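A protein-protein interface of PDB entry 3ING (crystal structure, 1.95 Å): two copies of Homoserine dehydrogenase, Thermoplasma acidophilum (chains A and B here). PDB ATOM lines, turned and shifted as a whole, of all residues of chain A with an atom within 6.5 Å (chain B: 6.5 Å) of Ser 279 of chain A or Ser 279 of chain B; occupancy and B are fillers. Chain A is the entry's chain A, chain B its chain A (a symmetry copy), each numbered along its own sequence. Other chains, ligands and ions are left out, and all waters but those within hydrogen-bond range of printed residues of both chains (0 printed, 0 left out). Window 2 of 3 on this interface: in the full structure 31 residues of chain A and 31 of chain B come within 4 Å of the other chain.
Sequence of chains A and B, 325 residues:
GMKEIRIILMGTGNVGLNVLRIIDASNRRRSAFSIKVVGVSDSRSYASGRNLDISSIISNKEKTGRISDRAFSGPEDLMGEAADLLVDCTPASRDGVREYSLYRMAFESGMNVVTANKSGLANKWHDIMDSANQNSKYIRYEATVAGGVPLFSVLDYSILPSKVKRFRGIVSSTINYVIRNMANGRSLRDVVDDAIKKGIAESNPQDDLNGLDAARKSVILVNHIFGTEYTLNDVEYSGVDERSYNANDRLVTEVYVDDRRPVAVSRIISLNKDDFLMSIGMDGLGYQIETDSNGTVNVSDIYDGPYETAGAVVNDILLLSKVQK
CE1 of Phe 276 of chain A touches CE1 of Phe 276 of chain B (3.8 Å).
Ser 279 of chain A touches Ser 279 of chain B.
Asn 298 of chain A touches Asn 298 of chain B.
Phe 276 of chain A touches its own counterpart, Phe 276 of chain B.
Ser 279 of chain A touches its own counterpart, Ser 279 of chain B.
Asn 298 of chain B touches its own counterpart, Asn 298 of chain A.
Asn 298 of chain A touches Ser 300 of chain B, and with the chains exchanged Ser 300 of chain A touches Asn 298 of chain B.
Positions printed for both chains: 273, 275, 276, 277, 278, 279, 280, 281, 298 and 300.
Lys 273 of chain A touches none of the printed residues of chain B.
Of the printed residues of chain B, Phe 276 of chain A touches Phe 276 (3.8 Å).
Ser 279 of chain A touches just one residue of chain B: Ser 279 (3.8 Å).
Of the printed residues of chain B, Ser 300 of chain A touches Asn 298 (2.8 Å).
Printed residues of chain A within 4 Å of Ser 279 of chain B: Ser 279.
Ile 280 of chain B touches none of the printed residues of chain A.
The nearest residue of chain B that does not touch Ser 279 of chain A is Phe 276 of chain B (4.4 Å).
The nearest residue of chain A that does not touch Ser 279 of chain B is Phe 276 of chain A (4.4 Å).
The backbone NH of Asn 298 of chain B is in hydrogen-bond range of the backbone carbonyl oxygen of Ser 300 of chain A, at 2.8 Å.
The backbone carbonyl oxygen (O) of Ser 300 of chain B sits at hydrogen-bond distance from the backbone NH (N) of Asn 298 of chain A (2.8 Å).
Printed residues of chain B that touch a printed residue of chain A: Phe 276, Ser 279, Asn 298 and Ser 300.
Hydrophobic or aromatic side chains of chain B that line the printed part of chain A: Phe 276.
The side-chain hydroxyl of Ser 279 of chain A is in hydrogen-bond range of the backbone carbonyl oxygen of Phe 276 of chain A, 2.8 Å away.
The backbone carbonyl oxygen (O) of Phe 276 of chain B is in hydrogen-bond range of the side-chain hydroxyl (OG) of Ser 279 of chain B, at 2.8 Å.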
ATOM      1  N   LYS A 273     -25.230  32.705   3.913  1.00  0.00           N
ATOM      2  CA  LYS A 273     -26.072  32.411   2.774  1.00  0.00           C
ATOM      3  C   LYS A 273     -25.491  31.343   1.886  1.00  0.00           C
ATOM      4  O   LYS A 273     -26.224  30.533   1.365  1.00  0.00           O
ATOM      5  CB  LYS A 273     -26.303  33.692   1.936  1.00  0.00           C
ATOM      6  N   ASP A 275     -23.465  28.856   2.742  1.00  0.00           N
ATOM      7  CA  ASP A 275     -23.159  27.620   3.448  1.00  0.00           C
ATOM      8  C   ASP A 275     -23.973  26.496   2.831  1.00  0.00           C
ATOM      9  O   ASP A 275     -25.156  26.684   2.612  1.00  0.00           O
ATOM     10  CB  ASP A 275     -23.571  27.820   4.903  1.00  0.00           C
ATOM     11  CG  ASP A 275     -23.078  26.719   5.835  1.00  0.00           C
ATOM     12  OD1 ASP A 275     -23.164  25.519   5.492  1.00  0.00           O
ATOM     13  OD2 ASP A 275     -22.634  27.086   6.944  1.00  0.00           O
ATOM     14  N   PHE A 276     -23.396  25.320   2.595  1.00  0.00           N
ATOM     15  CA  PHE A 276     -24.186  24.201   2.032  1.00  0.00           C
ATOM     16  C   PHE A 276     -25.397  23.886   2.888  1.00  0.00           C
ATOM     17  O   PHE A 276     -26.460  23.534   2.397  1.00  0.00           O
ATOM     18  CB  PHE A 276     -23.366  22.922   1.883  1.00  0.00           C
ATOM     19  CG  PHE A 276     -24.201  21.704   1.545  1.00  0.00           C
ATOM     20  CD1 PHE A 276     -24.721  21.549   0.276  1.00  0.00           C
ATOM     21  CD2 PHE A 276     -24.504  20.753   2.505  1.00  0.00           C
ATOM     22  CE1 PHE A 276     -25.541  20.483  -0.040  1.00  0.00           C
ATOM     23  CE2 PHE A 276     -25.300  19.680   2.203  1.00  0.00           C
ATOM     24  CZ  PHE A 276     -25.814  19.530   0.909  1.00  0.00           C
ATOM     25  N   LEU A 277     -25.237  24.042   4.182  1.00  0.00           N
ATOM     26  CA  LEU A 277     -26.299  23.640   5.100  1.00  0.00           C
ATOM     27  C   LEU A 277     -27.539  24.496   4.943  1.00  0.00           C
ATOM     28  O   LEU A 277     -28.641  24.097   5.356  1.00  0.00           O
ATOM     29  CB  LEU A 277     -25.792  23.650   6.555  1.00  0.00           C
ATOM     30  CG  LEU A 277     -24.689  22.647   6.906  1.00  0.00           C
ATOM     31  CD1 LEU A 277     -24.314  22.719   8.436  1.00  0.00           C
ATOM     32  CD2 LEU A 277     -25.115  21.237   6.441  1.00  0.00           C
ATOM     33  N   MET A 278     -27.371  25.688   4.389  1.00  0.00           N
ATOM     34  CA  MET A 278     -28.515  26.533   4.109  1.00  0.00           C
ATOM     35  C   MET A 278     -29.288  26.048   2.885  1.00  0.00           C
ATOM     36  O   MET A 278     -30.382  26.538   2.645  1.00  0.00           O
ATOM     37  CB  MET A 278     -28.067  27.995   3.913  1.00  0.00           C
ATOM     38  CG  MET A 278     -27.714  28.673   5.241  1.00  0.00           C
ATOM     39  SD  MET A 278     -29.241  28.912   6.438  1.00  0.00           S
ATOM     40  CE  MET A 278     -30.091  30.154   5.334  1.00  0.00           C
ATOM     41  N   SER A 279     -28.763  25.062   2.135  1.00  0.00           N
ATOM     42  CA  SER A 279     -29.517  24.523   1.006  1.00  0.00           C
ATOM     43  C   SER A 279     -30.556  23.502   1.493  1.00  0.00           C
ATOM     44  O   SER A 279     -31.423  23.098   0.739  1.00  0.00           O
ATOM     45  CB  SER A 279     -28.619  23.820  -0.024  1.00  0.00           C
ATOM     46  OG  SER A 279     -28.174  22.538   0.437  1.00  0.00           O
ATOM     47  N   ILE A 280     -30.435  23.077   2.748  1.00  0.00           N
ATOM     48  CA  ILE A 280     -31.315  22.046   3.271  1.00  0.00           C
ATOM     49  C   ILE A 280     -32.693  22.607   3.589  1.00  0.00           C
ATOM     50  O   ILE A 280     -32.848  23.574   4.356  1.00  0.00           O
ATOM     51  CB  ILE A 280     -30.697  21.356   4.477  1.00  0.00           C
ATOM     52  CG1 ILE A 280     -29.337  20.757   4.096  1.00  0.00           C
ATOM     53  CG2 ILE A 280     -31.649  20.259   5.040  1.00  0.00           C
ATOM     54  CD1 ILE A 280     -28.497  20.349   5.358  1.00  0.00           C
ATOM     55  N   GLY A 281     -33.698  21.965   3.014  1.00  0.00           N
ATOM     56  CA  GLY A 281     -35.079  22.419   3.125  1.00  0.00           C
ATOM     57  C   GLY A 281     -35.662  22.144   4.493  1.00  0.00           C
ATOM     58  O   GLY A 281     -35.101  21.400   5.310  1.00  0.00           O
ATOM     59  N   ASN A 298     -20.983  16.804   0.142  1.00  0.00           N
ATOM     60  CA  ASN A 298     -22.226  17.255   0.727  1.00  0.00           C
ATOM     61  C   ASN A 298     -23.337  16.251   0.452  1.00  0.00           C
ATOM     62  O   ASN A 298     -23.478  15.791  -0.656  1.00  0.00           O
ATOM     63  CB  ASN A 298     -22.637  18.622   0.174  1.00  0.00           C
ATOM     64  CG  ASN A 298     -21.470  19.586   0.057  1.00  0.00           C
ATOM     65  OD1 ASN A 298     -20.764  19.839   1.034  1.00  0.00           O
ATOM     66  ND2 ASN A 298     -21.272  20.145  -1.144  1.00  0.00           N
ATOM     67  N   SER A 300     -27.582  15.417   1.471  1.00  0.00           N
ATOM     68  CA  SER A 300     -28.814  15.844   2.122  1.00  0.00           C
ATOM     69  C   SER A 300     -30.007  15.080   1.559  1.00  0.00           C
ATOM     70  O   SER A 300     -29.869  14.264   0.652  1.00  0.00           O
ATOM     71  CB  SER A 300     -29.000  17.355   1.960  1.00  0.00           C
ATOM     72  OG  SER A 300     -29.202  17.731   0.623  1.00  0.00           O
ATOM     73  N   LYS B 273     -34.716  28.722  -8.678  1.00  0.00           N
ATOM     74  CA  LYS B 273     -33.907  29.128  -7.549  1.00  0.00           C
ATOM     75  C   LYS B 273     -33.852  28.079  -6.470  1.00  0.00           C
ATOM     76  O   LYS B 273     -32.822  27.900  -5.860  1.00  0.00           O
ATOM     77  CB  LYS B 273     -34.456  30.443  -6.945  1.00  0.00           C
ATOM     78  N   ASP B 275     -34.143  24.789  -6.806  1.00  0.00           N
ATOM     79  CA  ASP B 275     -33.688  23.491  -7.283  1.00  0.00           C
ATOM     80  C   ASP B 275     -32.423  23.115  -6.532  1.00  0.00           C
ATOM     81  O   ASP B 275     -31.548  23.952  -6.405  1.00  0.00           O
ATOM     82  CB  ASP B 275     -33.381  23.642  -8.770  1.00  0.00           C
ATOM     83  CG  ASP B 275     -33.145  22.315  -9.483  1.00  0.00           C
ATOM     84  OD1 ASP B 275     -32.434  21.434  -8.953  1.00  0.00           O
ATOM     85  OD2 ASP B 275     -33.662  22.192 -10.615  1.00  0.00           O
ATOM     86  N   PHE B 276     -32.274  21.872  -6.078  1.00  0.00           N
ATOM     87  CA  PHE B 276     -31.029  21.478  -5.378  1.00  0.00           C
ATOM     88  C   PHE B 276     -29.803  21.742  -6.229  1.00  0.00           C
ATOM     89  O   PHE B 276     -28.746  22.115  -5.741  1.00  0.00           O
ATOM     90  CB  PHE B 276     -31.022  20.004  -4.981  1.00  0.00           C
ATOM     91  CG  PHE B 276     -29.675  19.517  -4.490  1.00  0.00           C
ATOM     92  CD1 PHE B 276     -29.218  19.882  -3.240  1.00  0.00           C
ATOM     93  CD2 PHE B 276     -28.854  18.745  -5.295  1.00  0.00           C
ATOM     94  CE1 PHE B 276     -27.966  19.507  -2.795  1.00  0.00           C
ATOM     95  CE2 PHE B 276     -27.617  18.348  -4.861  1.00  0.00           C
ATOM     96  CZ  PHE B 276     -27.169  18.718  -3.587  1.00  0.00           C
ATOM     97  N   LEU B 277     -29.958  21.570  -7.522  1.00  0.00           N
ATOM     98  CA  LEU B 277     -28.805  21.671  -8.414  1.00  0.00           C
ATOM     99  C   LEU B 277     -28.245  23.077  -8.460  1.00  0.00           C
ATOM    100  O   LEU B 277     -27.085  23.284  -8.856  1.00  0.00           O
ATOM    101  CB  LEU B 277     -29.163  21.163  -9.824  1.00  0.00           C
ATOM    102  CG  LEU B 277     -29.519  19.679  -9.950  1.00  0.00           C
ATOM    103  CD1 LEU B 277     -29.796  19.281 -11.451  1.00  0.00           C
ATOM    104  CD2 LEU B 277     -28.415  18.830  -9.282  1.00  0.00           C
ATOM    105  N   MET B 278     -29.064  24.054  -8.102  1.00  0.00           N
ATOM    106  CA  MET B 278     -28.585  25.420  -8.020  1.00  0.00           C
ATOM    107  C   MET B 278     -27.734  25.645  -6.773  1.00  0.00           C
ATOM    108  O   MET B 278     -27.099  26.685  -6.671  1.00  0.00           O
ATOM    109  CB  MET B 278     -29.768  26.407  -8.045  1.00  0.00           C
ATOM    110  CG  MET B 278     -30.369  26.553  -9.447  1.00  0.00           C
ATOM    111  SD  MET B 278     -29.164  27.388 -10.740  1.00  0.00           S
ATOM    112  CE  MET B 278     -29.187  29.054  -9.899  1.00  0.00           C
ATOM    113  N   SER B 279     -27.670  24.671  -5.847  1.00  0.00           N
ATOM    114  CA  SER B 279     -26.800  24.826  -4.683  1.00  0.00           C
ATOM    115  C   SER B 279     -25.350  24.477  -5.047  1.00  0.00           C
ATOM    116  O   SER B 279     -24.442  24.743  -4.280  1.00  0.00           O
ATOM    117  CB  SER B 279     -27.218  23.927  -3.509  1.00  0.00           C
ATOM    118  OG  SER B 279     -26.865  22.556  -3.731  1.00  0.00           O
ATOM    119  N   ILE B 280     -25.157  23.856  -6.207  1.00  0.00           N
ATOM    120  CA  ILE B 280     -23.832  23.406  -6.597  1.00  0.00           C
ATOM    121  C   ILE B 280     -22.971  24.567  -7.070  1.00  0.00           C
ATOM    122  O   ILE B 280     -23.333  25.320  -7.992  1.00  0.00           O
ATOM    123  CB  ILE B 280     -23.911  22.303  -7.641  1.00  0.00           C
ATOM    124  CG1 ILE B 280     -24.739  21.130  -7.101  1.00  0.00           C
ATOM    125  CG2 ILE B 280     -22.488  21.831  -8.064  1.00  0.00           C
ATOM    126  CD1 ILE B 280     -25.156  20.128  -8.236  1.00  0.00           C
ATOM    127  N   GLY B 281     -21.808  24.684  -6.448  1.00  0.00           N
ATOM    128  CA  GLY B 281     -20.898  25.794  -6.699  1.00  0.00           C
ATOM    129  C   GLY B 281     -20.192  25.663  -8.031  1.00  0.00           C
ATOM    130  O   GLY B 281     -20.214  24.611  -8.687  1.00  0.00           O
ATOM    131  N   ASN B 298     -29.753  13.963  -2.146  1.00  0.00           N
ATOM    132  CA  ASN B 298     -28.933  14.918  -2.858  1.00  0.00           C
ATOM    133  C   ASN B 298     -27.469  14.747  -2.476  1.00  0.00           C
ATOM    134  O   ASN B 298     -27.153  14.627  -1.316  1.00  0.00           O
ATOM    135  CB  ASN B 298     -29.364  16.355  -2.557  1.00  0.00           C
ATOM    136  CG  ASN B 298     -30.872  16.528  -2.543  1.00  0.00           C
ATOM    137  OD1 ASN B 298     -31.552  16.189  -3.512  1.00  0.00           O
ATOM    138  ND2 ASN B 298     -31.403  17.076  -1.440  1.00  0.00           N
ATOM    139  N   SER B 300     -23.414  16.216  -3.553  1.00  0.00           N
ATOM    140  CA  SER B 300     -22.586  17.135  -4.325  1.00  0.00           C
ATOM    141  C   SER B 300     -21.199  17.252  -3.704  1.00  0.00           C
ATOM    142  O   SER B 300     -20.913  16.655  -2.669  1.00  0.00           O
ATOM    143  CB  SER B 300     -23.266  18.503  -4.422  1.00  0.00           C
ATOM    144  OG  SER B 300     -23.368  19.141  -3.177  1.00  0.00           O
